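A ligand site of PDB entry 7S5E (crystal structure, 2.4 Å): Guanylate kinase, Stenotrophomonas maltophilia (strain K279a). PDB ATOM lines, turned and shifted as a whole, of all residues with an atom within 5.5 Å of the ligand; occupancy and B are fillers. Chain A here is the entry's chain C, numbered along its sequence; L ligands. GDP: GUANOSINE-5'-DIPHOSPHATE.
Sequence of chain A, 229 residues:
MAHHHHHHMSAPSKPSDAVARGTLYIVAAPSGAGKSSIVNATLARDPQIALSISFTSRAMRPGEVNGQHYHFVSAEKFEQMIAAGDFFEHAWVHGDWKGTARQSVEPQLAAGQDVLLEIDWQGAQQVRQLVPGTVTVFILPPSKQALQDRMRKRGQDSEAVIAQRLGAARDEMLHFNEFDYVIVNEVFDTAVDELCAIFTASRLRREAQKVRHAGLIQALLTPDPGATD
N2 of the ligand lies within hydrogen-bond range of OD1 of Asp 120, 2.8 Å away.
NH2 of Arg 61 is in salt-bridge range of O3B of the ligand (3.1 Å).
OG1 of Thr 100 sits at hydrogen-bond distance from O6 of the ligand (3.4 Å).
The side-chain carboxylate (OE2) of Glu 89 is in hydrogen-bond range of a nitrogen (N1) of the ligand, 2.7 Å away.
The side-chain amino group (NZ) of Lys 98 is in salt-bridge range of an oxygen (O2B) of the ligand, at 2.9 Å.
An oxygen (O2B) of the ligand is in salt-bridge range of the guanidinium group (NE) of Arg 58 (3.1 Å).
O of Ile 119 lies close to O2' of the ligand.
O6 of the ligand sits at hydrogen-bond distance from OG of Ser 54 (2.5 Å).
The side-chain hydroxyl of Tyr 70 lies within hydrogen-bond range of an oxygen (O2A) of the ligand (2.5 Å).
O6 of the ligand lies close to N of Gly 99 (3.4 Å).
N of Asp 120 is in hydrogen-bond range of N3 of the ligand (3.0 Å).
A nitrogen (N7) of the ligand sits close to the backbone carbonyl oxygen (O) of Glu 118.
Residues that only touch the ligand: Ala 91 (3.7 Å), Val 93 (3.4 Å), Gly 123 (3.7 Å) and Glu 172 (3.8 Å).
Hydrophobic or aromatic side chains within 4 Å of the ligand: Tyr 70, Ala 91, Val 93 and Ile 119.
Within 4 Å of the ligand: Ser 54, Arg 58, Arg 61, Tyr 70, Glu 89, Ala 91, Val 93, Lys 98, Gly 99, Thr 100, Glu 118, Ile 119, Asp 120, Gly 123 and Glu 172.
O of Lys 98 is in hydrogen-bond range of N of Ala 91 (2.8 Å).
The backbone carbonyl oxygen (O) of Gly 99 lies within hydrogen-bond range of the backbone NH (N) of Phe 55 (2.8 Å).
The side-chain amino group (NZ) of Lys 35 is in salt-bridge range of the side-chain carboxylate (OE2) of Glu 118 (3.1 Å).
The side-chain carboxylate of Asp 120 is in hydrogen-bond range of the side-chain amide nitrogen of Gln 122 (2.8 Å).
OE2 of Glu 64 is in salt-bridge range of NH2 of Arg 61 (3.4 Å).
OE2 of Glu 64 lies within salt-bridge range of NH2 of Arg 58.
OE2 of Glu 89 is in hydrogen-bond range of OG1 of Thr 100 (2.7 Å).
OD1 of Asp 120 sits at hydrogen-bond distance from N of Gly 123, 2.9 Å away.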
ATOM      1  N   ALA A  29       1.906  10.380  17.426  1.00  0.00           N
ATOM      2  CA  ALA A  29       2.149  10.622  18.845  1.00  0.00           C
ATOM      3  C   ALA A  29       3.301   9.741  19.302  1.00  0.00           C
ATOM      4  O   ALA A  29       3.559   8.685  18.710  1.00  0.00           O
ATOM      5  CB  ALA A  29       0.902  10.318  19.680  1.00  0.00           C
ATOM      6  N   SER A  31       4.845   7.018  21.903  1.00  0.00           N
ATOM      7  CA  SER A  31       4.251   5.978  22.711  1.00  0.00           C
ATOM      8  C   SER A  31       3.947   6.506  24.104  1.00  0.00           C
ATOM      9  O   SER A  31       4.660   7.365  24.640  1.00  0.00           O
ATOM     10  CB  SER A  31       5.189   4.782  22.809  1.00  0.00           C
ATOM     11  OG  SER A  31       5.459   4.254  21.525  1.00  0.00           O
ATOM     12  N   LYS A  35      -2.434   7.352  22.203  1.00  0.00           N
ATOM     13  CA  LYS A  35      -2.934   7.578  20.855  1.00  0.00           C
ATOM     14  C   LYS A  35      -3.775   6.416  20.351  1.00  0.00           C
ATOM     15  O   LYS A  35      -4.825   6.629  19.724  1.00  0.00           O
ATOM     16  CB  LYS A  35      -1.758   7.841  19.907  1.00  0.00           C
ATOM     17  CG  LYS A  35      -2.167   7.998  18.463  1.00  0.00           C
ATOM     18  CD  LYS A  35      -0.948   8.023  17.552  1.00  0.00           C
ATOM     19  CE  LYS A  35      -0.234   6.689  17.530  1.00  0.00           C
ATOM     20  NZ  LYS A  35      -1.026   5.612  16.868  1.00  0.00           N
ATOM     21  N   SER A  54      -0.277  -0.892   7.980  1.00  0.00           N
ATOM     22  CA  SER A  54       1.038  -0.654   7.415  1.00  0.00           C
ATOM     23  C   SER A  54       1.772  -1.959   7.152  1.00  0.00           C
ATOM     24  O   SER A  54       1.499  -3.005   7.752  1.00  0.00           O
ATOM     25  CB  SER A  54       1.878   0.190   8.361  1.00  0.00           C
ATOM     26  OG  SER A  54       1.301   1.441   8.613  1.00  0.00           O
ATOM     27  N   PHE A  55       2.733  -1.890   6.242  1.00  0.00           N
ATOM     28  CA  PHE A  55       3.727  -2.932   6.076  1.00  0.00           C
ATOM     29  C   PHE A  55       4.927  -2.647   6.961  1.00  0.00           C
ATOM     30  O   PHE A  55       5.242  -1.497   7.250  1.00  0.00           O
ATOM     31  CB  PHE A  55       4.175  -3.036   4.616  1.00  0.00           C
ATOM     32  CG  PHE A  55       3.169  -3.692   3.733  1.00  0.00           C
ATOM     33  CD1 PHE A  55       2.032  -3.013   3.312  1.00  0.00           C
ATOM     34  CD2 PHE A  55       3.329  -5.006   3.331  1.00  0.00           C
ATOM     35  CE1 PHE A  55       1.102  -3.636   2.503  1.00  0.00           C
ATOM     36  CE2 PHE A  55       2.400  -5.629   2.521  1.00  0.00           C
ATOM     37  CZ  PHE A  55       1.280  -4.937   2.100  1.00  0.00           C
ATOM     38  N   ARG A  58       9.923  -5.564  10.381  1.00  0.00           N
ATOM     39  CA  ARG A  58      10.345  -5.982  11.699  1.00  0.00           C
ATOM     40  C   ARG A  58       9.916  -7.419  11.924  1.00  0.00           C
ATOM     41  O   ARG A  58       8.903  -7.889  11.400  1.00  0.00           O
ATOM     42  CB  ARG A  58       9.710  -5.073  12.763  1.00  0.00           C
ATOM     43  CG  ARG A  58       9.504  -5.728  14.099  1.00  0.00           C
ATOM     44  CD  ARG A  58       8.931  -4.783  15.152  1.00  0.00           C
ATOM     45  NE  ARG A  58       7.479  -4.623  15.097  1.00  0.00           N
ATOM     46  CZ  ARG A  58       6.608  -5.534  15.492  1.00  0.00           C
ATOM     47  NH1 ARG A  58       6.979  -6.740  15.875  1.00  0.00           N
ATOM     48  NH2 ARG A  58       5.315  -5.223  15.516  1.00  0.00           N
ATOM     49  N   ARG A  61       6.902 -10.731  16.737  1.00  0.00           N
ATOM     50  CA  ARG A  61       7.183 -11.271  18.055  1.00  0.00           C
ATOM     51  C   ARG A  61       6.265 -12.462  18.311  1.00  0.00           C
ATOM     52  O   ARG A  61       5.190 -12.546  17.715  1.00  0.00           O
ATOM     53  CB  ARG A  61       6.985 -10.198  19.124  1.00  0.00           C
ATOM     54  CG  ARG A  61       7.724  -8.894  18.843  1.00  0.00           C
ATOM     55  CD  ARG A  61       7.547  -7.879  19.958  1.00  0.00           C
ATOM     56  NE  ARG A  61       6.307  -7.118  19.817  1.00  0.00           N
ATOM     57  CZ  ARG A  61       6.199  -5.979  19.161  1.00  0.00           C
ATOM     58  NH1 ARG A  61       7.239  -5.414  18.573  1.00  0.00           N
ATOM     59  NH2 ARG A  61       5.005  -5.384  19.092  1.00  0.00           N
ATOM     60  N   GLU A  64       2.226 -12.742  17.763  1.00  0.00           N
ATOM     61  CA  GLU A  64       1.691 -11.748  16.840  1.00  0.00           C
ATOM     62  C   GLU A  64       0.977 -12.386  15.669  1.00  0.00           C
ATOM     63  O   GLU A  64       1.302 -13.494  15.230  1.00  0.00           O
ATOM     64  CB  GLU A  64       2.770 -10.813  16.300  1.00  0.00           C
ATOM     65  CG  GLU A  64       3.002  -9.577  17.148  1.00  0.00           C
ATOM     66  CD  GLU A  64       4.058  -8.659  16.577  1.00  0.00           C
ATOM     67  OE1 GLU A  64       5.070  -9.157  16.035  1.00  0.00           O
ATOM     68  OE2 GLU A  64       3.868  -7.432  16.634  1.00  0.00           O
ATOM     69  N   TYR A  70      -0.118  -5.111  11.663  1.00  0.00           N
ATOM     70  CA  TYR A  70       0.757  -4.837  10.532  1.00  0.00           C
ATOM     71  C   TYR A  70       0.631  -5.959   9.527  1.00  0.00           C
ATOM     72  O   TYR A  70       0.161  -7.059   9.848  1.00  0.00           O
ATOM     73  CB  TYR A  70       2.216  -4.771  10.961  1.00  0.00           C
ATOM     74  CG  TYR A  70       2.609  -3.553  11.749  1.00  0.00           C
ATOM     75  CD1 TYR A  70       2.832  -2.332  11.115  1.00  0.00           C
ATOM     76  CD2 TYR A  70       2.812  -3.636  13.112  1.00  0.00           C
ATOM     77  CE1 TYR A  70       3.228  -1.236  11.848  1.00  0.00           C
ATOM     78  CE2 TYR A  70       3.191  -2.556  13.837  1.00  0.00           C
ATOM     79  CZ  TYR A  70       3.406  -1.353  13.205  1.00  0.00           C
ATOM     80  OH  TYR A  70       3.805  -0.262  13.920  1.00  0.00           O
ATOM     81  N   GLU A  89       3.966   6.123   1.280  1.00  0.00           N
ATOM     82  CA  GLU A  89       5.086   6.626   2.046  1.00  0.00           C
ATOM     83  C   GLU A  89       5.787   5.426   2.663  1.00  0.00           C
ATOM     84  O   GLU A  89       5.179   4.377   2.904  1.00  0.00           O
ATOM     85  CB  GLU A  89       4.650   7.607   3.159  1.00  0.00           C
ATOM     86  CG  GLU A  89       3.743   7.003   4.235  1.00  0.00           C
ATOM     87  CD  GLU A  89       4.513   6.213   5.306  1.00  0.00           C
ATOM     88  OE1 GLU A  89       5.661   6.589   5.639  1.00  0.00           O
ATOM     89  OE2 GLU A  89       3.978   5.191   5.777  1.00  0.00           O
ATOM     90  N   HIS A  90       7.079   5.583   2.969  1.00  0.00           N
ATOM     91  CA  HIS A  90       7.798   4.579   3.742  1.00  0.00           C
ATOM     92  C   HIS A  90       8.953   5.278   4.437  1.00  0.00           C
ATOM     93  O   HIS A  90       9.367   6.372   4.050  1.00  0.00           O
ATOM     94  CB  HIS A  90       8.308   3.423   2.862  1.00  0.00           C
ATOM     95  CG  HIS A  90       9.428   3.809   1.952  1.00  0.00           C
ATOM     96  ND1 HIS A  90       9.229   4.273   0.671  1.00  0.00           N
ATOM     97  CD2 HIS A  90      10.776   3.868   2.163  1.00  0.00           C
ATOM     98  CE1 HIS A  90      10.387   4.564   0.117  1.00  0.00           C
ATOM     99  NE2 HIS A  90      11.343   4.339   1.003  1.00  0.00           N
ATOM    100  N   ALA A  91       9.445   4.641   5.503  1.00  0.00           N
ATOM    101  CA  ALA A  91      10.503   5.246   6.301  1.00  0.00           C
ATOM    102  C   ALA A  91      11.229   4.163   7.091  1.00  0.00           C
ATOM    103  O   ALA A  91      10.693   3.083   7.348  1.00  0.00           O
ATOM    104  CB  ALA A  91       9.946   6.301   7.249  1.00  0.00           C
ATOM    105  N   VAL A  93      12.136   3.345  10.557  1.00  0.00           N
ATOM    106  CA  VAL A  93      11.596   3.787  11.838  1.00  0.00           C
ATOM    107  C   VAL A  93      12.098   2.846  12.920  1.00  0.00           C
ATOM    108  O   VAL A  93      11.721   1.667  12.960  1.00  0.00           O
ATOM    109  CB  VAL A  93      10.059   3.847  11.815  1.00  0.00           C
ATOM    110  CG1 VAL A  93       9.525   4.287  13.169  1.00  0.00           C
ATOM    111  CG2 VAL A  93       9.564   4.755  10.689  1.00  0.00           C
ATOM    112  N   HIS A  94      12.932   3.372  13.822  1.00  0.00           N
ATOM    113  CA  HIS A  94      13.436   2.619  14.966  1.00  0.00           C
ATOM    114  C   HIS A  94      14.071   1.292  14.552  1.00  0.00           C
ATOM    115  O   HIS A  94      13.818   0.249  15.164  1.00  0.00           O
ATOM    116  CB  HIS A  94      12.318   2.377  15.999  1.00  0.00           C
ATOM    117  CG  HIS A  94      11.677   3.632  16.501  1.00  0.00           C
ATOM    118  ND1 HIS A  94      12.342   4.835  16.614  1.00  0.00           N
ATOM    119  CD2 HIS A  94      10.415   3.862  16.938  1.00  0.00           C
ATOM    120  CE1 HIS A  94      11.532   5.743  17.100  1.00  0.00           C
ATOM    121  NE2 HIS A  94      10.348   5.194  17.306  1.00  0.00           N
ATOM    122  N   LYS A  98       9.054   0.626   7.827  1.00  0.00           N
ATOM    123  CA  LYS A  98       7.623   0.829   7.961  1.00  0.00           C
ATOM    124  C   LYS A  98       7.141   1.594   6.745  1.00  0.00           C
ATOM    125  O   LYS A  98       7.821   2.515   6.272  1.00  0.00           O
ATOM    126  CB  LYS A  98       7.279   1.633   9.217  1.00  0.00           C
ATOM    127  CG  LYS A  98       7.578   0.942  10.560  1.00  0.00           C
ATOM    128  CD  LYS A  98       6.419   0.050  10.989  1.00  0.00           C
ATOM    129  CE  LYS A  98       6.669  -0.690  12.306  1.00  0.00           C
ATOM    130  NZ  LYS A  98       6.681   0.196  13.515  1.00  0.00           N
ATOM    131  N   GLY A  99       5.959   1.265   6.252  1.00  0.00           N
ATOM    132  CA  GLY A  99       5.458   1.954   5.071  1.00  0.00           C
ATOM    133  C   GLY A  99       3.984   1.709   4.865  1.00  0.00           C
ATOM    134  O   GLY A  99       3.436   0.683   5.284  1.00  0.00           O
ATOM    135  N   THR A 100       3.345   2.654   4.168  1.00  0.00           N
ATOM    136  CA  THR A 100       1.942   2.574   3.811  1.00  0.00           C
ATOM    137  C   THR A 100       1.821   2.297   2.321  1.00  0.00           C
ATOM    138  O   THR A 100       2.258   3.096   1.496  1.00  0.00           O
ATOM    139  CB  THR A 100       1.231   3.891   4.146  1.00  0.00           C
ATOM    140  OG1 THR A 100       1.434   4.223   5.520  1.00  0.00           O
ATOM    141  CG2 THR A 100      -0.258   3.794   3.844  1.00  0.00           C
ATOM    142  N   GLU A 118      -1.614   5.868  10.895  1.00  0.00           N
ATOM    143  CA  GLU A 118      -0.852   5.918  12.151  1.00  0.00           C
ATOM    144  C   GLU A 118       0.606   5.704  11.765  1.00  0.00           C
ATOM    145  O   GLU A 118       1.083   4.579  11.720  1.00  0.00           O
ATOM    146  CB  GLU A 118      -1.304   4.847  13.116  1.00  0.00           C
ATOM    147  CG  GLU A 118      -2.685   5.021  13.685  1.00  0.00           C
ATOM    148  CD  GLU A 118      -3.031   3.895  14.614  1.00  0.00           C
ATOM    149  OE1 GLU A 118      -2.804   2.719  14.231  1.00  0.00           O
ATOM    150  OE2 GLU A 118      -3.501   4.168  15.745  1.00  0.00           O
ATOM    151  N   ILE A 119       1.312   6.799  11.474  1.00  0.00           N
ATOM    152  CA  ILE A 119       2.677   6.723  10.974  1.00  0.00           C
ATOM    153  C   ILE A 119       3.535   7.692  11.781  1.00  0.00           C
ATOM    154  O   ILE A 119       3.030   8.505  12.562  1.00  0.00           O
ATOM    155  CB  ILE A 119       2.780   7.030   9.465  1.00  0.00           C
ATOM    156  CG1 ILE A 119       2.365   8.464   9.181  1.00  0.00           C
ATOM    157  CG2 ILE A 119       1.877   6.098   8.685  1.00  0.00           C
ATOM    158  CD1 ILE A 119       2.270   8.791   7.705  1.00  0.00           C
ATOM    159  N   ASP A 120       4.847   7.610  11.565  1.00  0.00           N
ATOM    160  CA  ASP A 120       5.766   8.488  12.265  1.00  0.00           C
ATOM    161  C   ASP A 120       5.867   9.840  11.535  1.00  0.00           C
ATOM    162  O   ASP A 120       5.190  10.081  10.524  1.00  0.00           O
ATOM    163  CB  ASP A 120       7.143   7.821  12.423  1.00  0.00           C
ATOM    164  CG  ASP A 120       8.069   8.028  11.231  1.00  0.00           C
ATOM    165  OD1 ASP A 120       7.610   8.029  10.062  1.00  0.00           O
ATOM    166  OD2 ASP A 120       9.282   8.179  11.477  1.00  0.00           O
ATOM    167  N   GLN A 122       8.368  11.104   9.866  1.00  0.00           N
ATOM    168  CA  GLN A 122       8.948  10.959   8.534  1.00  0.00           C
ATOM    169  C   GLN A 122       7.888  10.639   7.498  1.00  0.00           C
ATOM    170  O   GLN A 122       7.875  11.214   6.400  1.00  0.00           O
ATOM    171  CB  GLN A 122      10.033   9.880   8.542  1.00  0.00           C
ATOM    172  CG  GLN A 122      11.179  10.138   9.520  1.00  0.00           C
ATOM    173  CD  GLN A 122      12.150   8.977   9.583  1.00  0.00           C
ATOM    174  OE1 GLN A 122      13.187   8.982   8.913  1.00  0.00           O
ATOM    175  NE2 GLN A 122      11.823   7.991  10.401  1.00  0.00           N
ATOM    176  N   GLY A 123       6.999   9.703   7.824  1.00  0.00           N
ATOM    177  CA  GLY A 123       5.897   9.402   6.913  1.00  0.00           C
ATOM    178  C   GLY A 123       4.931  10.559   6.769  1.00  0.00           C
ATOM    179  O   GLY A 123       4.460  10.845   5.669  1.00  0.00           O
ATOM    180  N   GLU A 172      10.280  12.082  18.984  1.00  0.00           N
ATOM    181  CA  GLU A 172       9.071  12.192  18.165  1.00  0.00           C
ATOM    182  C   GLU A 172       8.339  13.508  18.436  1.00  0.00           C
ATOM    183  O   GLU A 172       7.915  14.191  17.502  1.00  0.00           O
ATOM    184  CB  GLU A 172       8.160  10.984  18.405  1.00  0.00           C
ATOM    185  CG  GLU A 172       6.967  10.907  17.443  1.00  0.00           C
ATOM    186  CD  GLU A 172       7.249  10.026  16.218  1.00  0.00           C
ATOM    187  OE1 GLU A 172       8.439   9.727  15.973  1.00  0.00           O
ATOM    188  OE2 GLU A 172       6.287   9.657  15.503  1.00  0.00           O
HETATM  189  PB  GDP L   1       6.194  -1.731  17.191  1.00  0.00           P
HETATM  190  O1B GDP L   1       7.479  -2.043  18.023  1.00  0.00           O
HETATM  191  O2B GDP L   1       6.595  -1.687  15.683  1.00  0.00           O
HETATM  192  O3B GDP L   1       5.026  -2.687  17.479  1.00  0.00           O
HETATM  193  O3A GDP L   1       5.762  -0.238  17.562  1.00  0.00           O
HETATM  194  PA  GDP L   1       4.555   0.638  16.987  1.00  0.00           P
HETATM  195  O1A GDP L   1       4.064   1.539  18.142  1.00  0.00           O
HETATM  196  O2A GDP L   1       3.522  -0.248  16.388  1.00  0.00           O
HETATM  197  O5' GDP L   1       5.235   1.638  15.909  1.00  0.00           O
HETATM  198  C5' GDP L   1       6.520   2.285  16.045  1.00  0.00           C
HETATM  199  C4' GDP L   1       6.504   3.572  15.264  1.00  0.00           C
HETATM  200  O4' GDP L   1       6.307   3.289  13.859  1.00  0.00           O
HETATM  201  C3' GDP L   1       5.440   4.596  15.663  1.00  0.00           C
HETATM  202  O3' GDP L   1       6.004   5.877  15.891  1.00  0.00           O
HETATM  203  C2' GDP L   1       4.489   4.622  14.460  1.00  0.00           C
HETATM  204  O2' GDP L   1       3.970   5.924  14.234  1.00  0.00           O
HETATM  205  C1' GDP L   1       5.433   4.260  13.323  1.00  0.00           C
HETATM  206  N9  GDP L   1       4.756   3.682  12.153  1.00  0.00           N
HETATM  207  C8  GDP L   1       3.795   2.707  12.170  1.00  0.00           C
HETATM  208  N7  GDP L   1       3.356   2.403  10.968  1.00  0.00           N
HETATM  209  C5  GDP L   1       4.059   3.239  10.115  1.00  0.00           C
HETATM  210  C6  GDP L   1       4.009   3.407   8.680  1.00  0.00           C
HETATM  211  O6  GDP L   1       3.328   2.768   7.873  1.00  0.00           O
HETATM  212  N1  GDP L   1       4.858   4.400   8.243  1.00  0.00           N
HETATM  213  C2  GDP L   1       5.692   5.134   9.047  1.00  0.00           C
HETATM  214  N2  GDP L   1       6.437   6.058   8.438  1.00  0.00           N
HETATM  215  N3  GDP L   1       5.772   4.978  10.370  1.00  0.00           N
HETATM  216  C4  GDP L   1       4.928   4.032  10.828  1.00  0.00           C
